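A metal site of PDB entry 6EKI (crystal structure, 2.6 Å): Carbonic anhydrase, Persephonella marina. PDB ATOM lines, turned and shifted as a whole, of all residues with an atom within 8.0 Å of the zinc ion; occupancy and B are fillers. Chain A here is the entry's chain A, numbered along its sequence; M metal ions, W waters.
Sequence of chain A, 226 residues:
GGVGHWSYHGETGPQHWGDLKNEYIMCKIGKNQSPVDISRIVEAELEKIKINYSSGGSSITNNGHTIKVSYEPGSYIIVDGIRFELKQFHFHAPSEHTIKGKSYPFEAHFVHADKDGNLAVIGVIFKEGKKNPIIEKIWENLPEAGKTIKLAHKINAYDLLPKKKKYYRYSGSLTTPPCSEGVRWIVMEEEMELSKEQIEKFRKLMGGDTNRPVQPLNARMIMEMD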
ATOM      1  N   TYR A   8     -14.744  -9.930  21.084  1.00  0.00           N
ATOM      2  CA  TYR A   8     -13.528  -9.137  20.896  1.00  0.00           C
ATOM      3  C   TYR A   8     -12.441  -9.918  20.186  1.00  0.00           C
ATOM      4  O   TYR A   8     -11.355  -9.400  19.971  1.00  0.00           O
ATOM      5  CB  TYR A   8     -13.017  -8.655  22.228  1.00  0.00           C
ATOM      6  CG  TYR A   8     -13.900  -7.588  22.792  1.00  0.00           C
ATOM      7  CD1 TYR A   8     -13.871  -6.309  22.287  1.00  0.00           C
ATOM      8  CD2 TYR A   8     -14.800  -7.867  23.808  1.00  0.00           C
ATOM      9  CE1 TYR A   8     -14.697  -5.339  22.784  1.00  0.00           C
ATOM     10  CE2 TYR A   8     -15.635  -6.897  24.319  1.00  0.00           C
ATOM     11  CZ  TYR A   8     -15.578  -5.630  23.804  1.00  0.00           C
ATOM     12  OH  TYR A   8     -16.399  -4.641  24.311  1.00  0.00           O
ATOM     13  N   THR A  66     -19.280  -7.624  29.383  1.00  0.00           N
ATOM     14  CA  THR A  66     -18.878  -6.635  30.377  1.00  0.00           C
ATOM     15  C   THR A  66     -19.634  -6.932  31.637  1.00  0.00           C
ATOM     16  O   THR A  66     -20.472  -7.829  31.649  1.00  0.00           O
ATOM     17  CB  THR A  66     -19.199  -5.189  29.935  1.00  0.00           C
ATOM     18  OG1 THR A  66     -18.539  -4.246  30.772  1.00  0.00           O
ATOM     19  CG2 THR A  66     -20.708  -4.913  29.908  1.00  0.00           C
ATOM     20  N   GLN A  88     -27.201   3.216  32.765  1.00  0.00           N
ATOM     21  CA  GLN A  88     -26.335   2.129  33.201  1.00  0.00           C
ATOM     22  C   GLN A  88     -24.904   2.555  33.106  1.00  0.00           C
ATOM     23  O   GLN A  88     -24.573   3.477  32.357  1.00  0.00           O
ATOM     24  CB  GLN A  88     -26.536   0.898  32.315  1.00  0.00           C
ATOM     25  CG  GLN A  88     -26.390   1.217  30.851  1.00  0.00           C
ATOM     26  CD  GLN A  88     -25.082   0.731  30.248  1.00  0.00           C
ATOM     27  OE1 GLN A  88     -24.096   0.514  30.949  1.00  0.00           O
ATOM     28  NE2 GLN A  88     -25.068   0.619  28.919  1.00  0.00           N
ATOM     29  N   PHE A  89     -24.062   1.790  33.766  1.00  0.00           N
ATOM     30  CA  PHE A  89     -22.629   1.950  33.585  1.00  0.00           C
ATOM     31  C   PHE A  89     -21.912   0.600  33.618  1.00  0.00           C
ATOM     32  O   PHE A  89     -22.301  -0.301  34.350  1.00  0.00           O
ATOM     33  CB  PHE A  89     -22.061   2.929  34.652  1.00  0.00           C
ATOM     34  CG  PHE A  89     -22.138   2.412  36.068  1.00  0.00           C
ATOM     35  CD1 PHE A  89     -23.289   2.530  36.802  1.00  0.00           C
ATOM     36  CD2 PHE A  89     -21.036   1.835  36.666  1.00  0.00           C
ATOM     37  CE1 PHE A  89     -23.353   2.060  38.083  1.00  0.00           C
ATOM     38  CE2 PHE A  89     -21.107   1.377  37.977  1.00  0.00           C
ATOM     39  CZ  PHE A  89     -22.261   1.496  38.661  1.00  0.00           C
ATOM     40  N   HIS A  90     -20.857   0.483  32.814  1.00  0.00           N
ATOM     41  CA  HIS A  90     -20.140  -0.755  32.642  1.00  0.00           C
ATOM     42  C   HIS A  90     -18.640  -0.538  32.520  1.00  0.00           C
ATOM     43  O   HIS A  90     -18.180   0.590  32.581  1.00  0.00           O
ATOM     44  CB  HIS A  90     -20.652  -1.475  31.430  1.00  0.00           C
ATOM     45  CG  HIS A  90     -20.605  -0.649  30.185  1.00  0.00           C
ATOM     46  ND1 HIS A  90     -21.693   0.059  29.715  1.00  0.00           N
ATOM     47  CD2 HIS A  90     -19.585  -0.378  29.337  1.00  0.00           C
ATOM     48  CE1 HIS A  90     -21.358   0.698  28.620  1.00  0.00           C
ATOM     49  NE2 HIS A  90     -20.084   0.450  28.364  1.00  0.00           N
ATOM     50  N   PHE A  91     -17.879  -1.603  32.302  1.00  0.00           N
ATOM     51  CA  PHE A  91     -16.424  -1.494  32.328  1.00  0.00           C
ATOM     52  C   PHE A  91     -15.744  -2.185  31.127  1.00  0.00           C
ATOM     53  O   PHE A  91     -16.301  -3.083  30.510  1.00  0.00           O
ATOM     54  CB  PHE A  91     -15.884  -2.111  33.628  1.00  0.00           C
ATOM     55  CG  PHE A  91     -16.562  -1.625  34.875  1.00  0.00           C
ATOM     56  CD1 PHE A  91     -16.184  -0.446  35.477  1.00  0.00           C
ATOM     57  CD2 PHE A  91     -17.570  -2.359  35.441  1.00  0.00           C
ATOM     58  CE1 PHE A  91     -16.831   0.021  36.620  1.00  0.00           C
ATOM     59  CE2 PHE A  91     -18.221  -1.917  36.601  1.00  0.00           C
ATOM     60  CZ  PHE A  91     -17.842  -0.730  37.197  1.00  0.00           C
ATOM     61  N   HIS A  92     -14.554  -1.723  30.793  1.00  0.00           N
ATOM     62  CA  HIS A  92     -13.725  -2.336  29.780  1.00  0.00           C
ATOM     63  C   HIS A  92     -12.348  -2.414  30.365  1.00  0.00           C
ATOM     64  O   HIS A  92     -11.958  -1.586  31.189  1.00  0.00           O
ATOM     65  CB  HIS A  92     -13.640  -1.520  28.497  1.00  0.00           C
ATOM     66  CG  HIS A  92     -14.980  -1.208  27.913  1.00  0.00           C
ATOM     67  ND1 HIS A  92     -15.621  -2.049  27.049  1.00  0.00           N
ATOM     68  CD2 HIS A  92     -15.774  -0.144  28.087  1.00  0.00           C
ATOM     69  CE1 HIS A  92     -16.798  -1.521  26.724  1.00  0.00           C
ATOM     70  NE2 HIS A  92     -16.906  -0.373  27.347  1.00  0.00           N
ATOM     71  N   GLU A  96     -10.558   1.652  26.659  1.00  0.00           N
ATOM     72  CA  GLU A  96     -10.899   1.775  25.247  1.00  0.00           C
ATOM     73  C   GLU A  96     -10.219   3.006  24.669  1.00  0.00           C
ATOM     74  O   GLU A  96      -9.556   2.936  23.639  1.00  0.00           O
ATOM     75  CB  GLU A  96     -12.403   1.829  25.041  1.00  0.00           C
ATOM     76  CG  GLU A  96     -13.060   0.515  25.413  1.00  0.00           C
ATOM     77  CD  GLU A  96     -14.238   0.150  24.531  1.00  0.00           C
ATOM     78  OE1 GLU A  96     -15.279   0.785  24.614  1.00  0.00           O
ATOM     79  OE2 GLU A  96     -14.130  -0.796  23.739  1.00  0.00           O
ATOM     80  N   HIS A  97     -10.359   4.130  25.353  1.00  0.00           N
ATOM     81  CA  HIS A  97      -9.624   5.328  24.961  1.00  0.00           C
ATOM     82  C   HIS A  97      -8.185   5.281  25.449  1.00  0.00           C
ATOM     83  O   HIS A  97      -7.890   4.823  26.536  1.00  0.00           O
ATOM     84  CB  HIS A  97     -10.285   6.578  25.549  1.00  0.00           C
ATOM     85  CG  HIS A  97     -11.653   6.835  25.021  1.00  0.00           C
ATOM     86  ND1 HIS A  97     -12.771   6.264  25.579  1.00  0.00           N
ATOM     87  CD2 HIS A  97     -12.085   7.604  24.001  1.00  0.00           C
ATOM     88  CE1 HIS A  97     -13.843   6.653  24.922  1.00  0.00           C
ATOM     89  NE2 HIS A  97     -13.455   7.466  23.954  1.00  0.00           N
ATOM     90  N   GLU A 107     -11.434   0.912  32.278  1.00  0.00           N
ATOM     91  CA  GLU A 107     -12.224   2.095  31.920  1.00  0.00           C
ATOM     92  C   GLU A 107     -13.659   1.876  32.292  1.00  0.00           C
ATOM     93  O   GLU A 107     -14.157   0.766  32.212  1.00  0.00           O
ATOM     94  CB  GLU A 107     -12.117   2.384  30.423  1.00  0.00           C
ATOM     95  CG  GLU A 107     -12.917   3.589  29.976  1.00  0.00           C
ATOM     96  CD  GLU A 107     -12.649   4.008  28.504  1.00  0.00           C
ATOM     97  OE1 GLU A 107     -11.567   3.660  27.935  1.00  0.00           O
ATOM     98  OE2 GLU A 107     -13.526   4.682  27.916  1.00  0.00           O
ATOM     99  N   ALA A 108     -14.305   2.928  32.769  1.00  0.00           N
ATOM    100  CA  ALA A 108     -15.733   2.849  33.127  1.00  0.00           C
ATOM    101  C   ALA A 108     -16.520   3.754  32.195  1.00  0.00           C
ATOM    102  O   ALA A 108     -16.076   4.851  31.908  1.00  0.00           O
ATOM    103  CB  ALA A 108     -15.967   3.254  34.566  1.00  0.00           C
ATOM    104  N   HIS A 109     -17.641   3.258  31.705  1.00  0.00           N
ATOM    105  CA  HIS A 109     -18.560   4.042  30.885  1.00  0.00           C
ATOM    106  C   HIS A 109     -19.922   4.300  31.525  1.00  0.00           C
ATOM    107  O   HIS A 109     -20.616   3.362  31.886  1.00  0.00           O
ATOM    108  CB  HIS A 109     -18.770   3.335  29.553  1.00  0.00           C
ATOM    109  CG  HIS A 109     -17.579   3.410  28.648  1.00  0.00           C
ATOM    110  ND1 HIS A 109     -17.415   2.558  27.591  1.00  0.00           N
ATOM    111  CD2 HIS A 109     -16.517   4.251  28.642  1.00  0.00           C
ATOM    112  CE1 HIS A 109     -16.294   2.862  26.961  1.00  0.00           C
ATOM    113  NE2 HIS A 109     -15.732   3.888  27.584  1.00  0.00           N
ATOM    114  N   PHE A 110     -20.335   5.552  31.613  1.00  0.00           N
ATOM    115  CA  PHE A 110     -21.659   5.875  32.162  1.00  0.00           C
ATOM    116  C   PHE A 110     -22.582   6.317  31.052  1.00  0.00           C
ATOM    117  O   PHE A 110     -22.354   7.352  30.431  1.00  0.00           O
ATOM    118  CB  PHE A 110     -21.543   6.930  33.266  1.00  0.00           C
ATOM    119  CG  PHE A 110     -20.602   6.531  34.355  1.00  0.00           C
ATOM    120  CD1 PHE A 110     -19.244   6.717  34.208  1.00  0.00           C
ATOM    121  CD2 PHE A 110     -21.071   5.930  35.487  1.00  0.00           C
ATOM    122  CE1 PHE A 110     -18.359   6.311  35.226  1.00  0.00           C
ATOM    123  CE2 PHE A 110     -20.215   5.543  36.472  1.00  0.00           C
ATOM    124  CZ  PHE A 110     -18.844   5.730  36.348  1.00  0.00           C
ATOM    125  N   VAL A 111     -23.542   5.460  30.737  1.00  0.00           N
ATOM    126  CA  VAL A 111     -24.390   5.679  29.596  1.00  0.00           C
ATOM    127  C   VAL A 111     -25.704   6.350  29.957  1.00  0.00           C
ATOM    128  O   VAL A 111     -26.514   5.826  30.730  1.00  0.00           O
ATOM    129  CB  VAL A 111     -24.630   4.366  28.862  1.00  0.00           C
ATOM    130  CG1 VAL A 111     -25.359   4.641  27.620  1.00  0.00           C
ATOM    131  CG2 VAL A 111     -23.306   3.693  28.501  1.00  0.00           C
ATOM    132  N   VAL A 121     -22.125   9.708  26.841  1.00  0.00           N
ATOM    133  CA  VAL A 121     -21.347   8.749  27.614  1.00  0.00           C
ATOM    134  C   VAL A 121     -20.197   9.426  28.318  1.00  0.00           C
ATOM    135  O   VAL A 121     -19.456  10.216  27.717  1.00  0.00           O
ATOM    136  CB  VAL A 121     -20.812   7.562  26.746  1.00  0.00           C
ATOM    137  CG1 VAL A 121     -20.237   6.485  27.620  1.00  0.00           C
ATOM    138  CG2 VAL A 121     -21.947   6.935  25.942  1.00  0.00           C
ATOM    139  N   ILE A 122     -20.084   9.122  29.606  1.00  0.00           N
ATOM    140  CA  ILE A 122     -18.991   9.599  30.401  1.00  0.00           C
ATOM    141  C   ILE A 122     -17.994   8.462  30.461  1.00  0.00           C
ATOM    142  O   ILE A 122     -18.336   7.315  30.737  1.00  0.00           O
ATOM    143  CB  ILE A 122     -19.411  10.047  31.822  1.00  0.00           C
ATOM    144  CG1 ILE A 122     -20.114  11.368  31.771  1.00  0.00           C
ATOM    145  CG2 ILE A 122     -18.206  10.298  32.693  1.00  0.00           C
ATOM    146  CD1 ILE A 122     -20.749  11.832  33.149  1.00  0.00           C
ATOM    147  N   SER A 173     -19.126   7.470  18.769  1.00  0.00           N
ATOM    148  CA  SER A 173     -20.099   6.405  18.629  1.00  0.00           C
ATOM    149  C   SER A 173     -20.145   5.495  19.846  1.00  0.00           C
ATOM    150  O   SER A 173     -19.343   5.612  20.769  1.00  0.00           O
ATOM    151  CB  SER A 173     -19.759   5.555  17.411  1.00  0.00           C
ATOM    152  OG  SER A 173     -18.625   4.764  17.744  1.00  0.00           O
ATOM    153  N   LEU A 174     -21.109   4.583  19.845  1.00  0.00           N
ATOM    154  CA  LEU A 174     -21.049   3.440  20.721  1.00  0.00           C
ATOM    155  C   LEU A 174     -19.815   2.626  20.354  1.00  0.00           C
ATOM    156  O   LEU A 174     -19.440   2.587  19.185  1.00  0.00           O
ATOM    157  CB  LEU A 174     -22.267   2.577  20.562  1.00  0.00           C
ATOM    158  CG  LEU A 174     -23.635   3.164  20.832  1.00  0.00           C
ATOM    159  CD1 LEU A 174     -24.693   2.179  20.342  1.00  0.00           C
ATOM    160  CD2 LEU A 174     -23.777   3.365  22.285  1.00  0.00           C
ATOM    161  N   THR A 175     -19.152   2.044  21.355  1.00  0.00           N
ATOM    162  CA  THR A 175     -17.928   1.247  21.127  1.00  0.00           C
ATOM    163  C   THR A 175     -18.172  -0.237  20.938  1.00  0.00           C
ATOM    164  O   THR A 175     -17.213  -1.002  20.779  1.00  0.00           O
ATOM    165  CB  THR A 175     -16.906   1.433  22.242  1.00  0.00           C
ATOM    166  OG1 THR A 175     -17.521   1.128  23.505  1.00  0.00           O
ATOM    167  CG2 THR A 175     -16.413   2.899  22.207  1.00  0.00           C
ATOM    168  N   THR A 176     -19.437  -0.622  20.922  1.00  0.00           N
ATOM    169  CA  THR A 176     -19.836  -1.981  20.614  1.00  0.00           C
ATOM    170  C   THR A 176     -20.941  -1.861  19.621  1.00  0.00           C
ATOM    171  O   THR A 176     -21.607  -0.815  19.596  1.00  0.00           O
ATOM    172  CB  THR A 176     -20.337  -2.711  21.820  1.00  0.00           C
ATOM    173  OG1 THR A 176     -21.461  -2.000  22.326  1.00  0.00           O
ATOM    174  CG2 THR A 176     -19.243  -2.798  22.854  1.00  0.00           C
ATOM    175  N   TRP A 185     -19.313  12.228  23.680  1.00  0.00           N
ATOM    176  CA  TRP A 185     -18.353  11.616  24.605  1.00  0.00           C
ATOM    177  C   TRP A 185     -17.803  12.651  25.524  1.00  0.00           C
ATOM    178  O   TRP A 185     -17.352  13.715  25.110  1.00  0.00           O
ATOM    179  CB  TRP A 185     -17.211  10.908  23.870  1.00  0.00           C
ATOM    180  CG  TRP A 185     -17.602   9.478  23.587  1.00  0.00           C
ATOM    181  CD1 TRP A 185     -18.153   9.004  22.443  1.00  0.00           C
ATOM    182  CD2 TRP A 185     -17.516   8.356  24.480  1.00  0.00           C
ATOM    183  NE1 TRP A 185     -18.423   7.654  22.563  1.00  0.00           N
ATOM    184  CE2 TRP A 185     -18.039   7.240  23.813  1.00  0.00           C
ATOM    185  CE3 TRP A 185     -17.046   8.193  25.782  1.00  0.00           C
ATOM    186  CZ2 TRP A 185     -18.109   5.987  24.395  1.00  0.00           C
ATOM    187  CZ3 TRP A 185     -17.118   6.933  26.370  1.00  0.00           C
ATOM    188  CH2 TRP A 185     -17.624   5.854  25.673  1.00  0.00           C
ATOM    189  N   THR A 210     -11.229  -6.637  26.612  1.00  0.00           N
ATOM    190  CA  THR A 210     -12.585  -6.216  26.239  1.00  0.00           C
ATOM    191  C   THR A 210     -12.658  -4.779  25.704  1.00  0.00           C
ATOM    192  O   THR A 210     -13.628  -4.090  25.945  1.00  0.00           O
ATOM    193  CB  THR A 210     -13.581  -6.358  27.400  1.00  0.00           C
ATOM    194  OG1 THR A 210     -13.046  -5.772  28.591  1.00  0.00           O
ATOM    195  CG2 THR A 210     -13.898  -7.818  27.633  1.00  0.00           C
HETATM  196 ZN    ZN M   1     -18.513   0.879  26.919  1.00  0.00          ZN
HETATM  197  O   HOH W   1     -20.198   2.484  25.110  1.00  0.00           O
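The side-chain carboxylate of Glu 96 lies close to a ring nitrogen (NE2) of His 92, at 3.4 Å.
O of His 92 lies within hydrogen-bond range of N of Glu 107 (2.8 Å).
ND1 of His 92 sits at hydrogen-bond distance from O of Thr 210 (3.1 Å).
A ring nitrogen (ND1) of His 90 lies within hydrogen-bond range of the side-chain amide oxygen (OE1) of Gln 88, at 2.7 Å.
OG1 of Thr 175 is in hydrogen-bond range of OE1 of Glu 96.
The backbone NH (N) of Glu 96 sits at hydrogen-bond distance from the side-chain carboxylate (OE1) of Glu 107.
OE1 of Glu 96 touches the zinc ion, at 3.97 Å.
Thr 175 touches the zinc ion (OG1 to ZN, 3.6 Å).
Five residues have an atom within 4 Å of the zinc ion: His 90, His 92, Glu 96, His 109 and Thr 175.
The nearest printed residue that does not touch the zinc ion is Trp 185 (5.2 Å).
The zinc ion is bound by a ring nitrogen (NE2) of His 92 (2.1 Å), a ring nitrogen (ND1) of His 109 (2.1 Å) and a ring nitrogen (NE2) of His 90 (2.2 Å).
The zinc ion has three donor atoms within binding distance.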
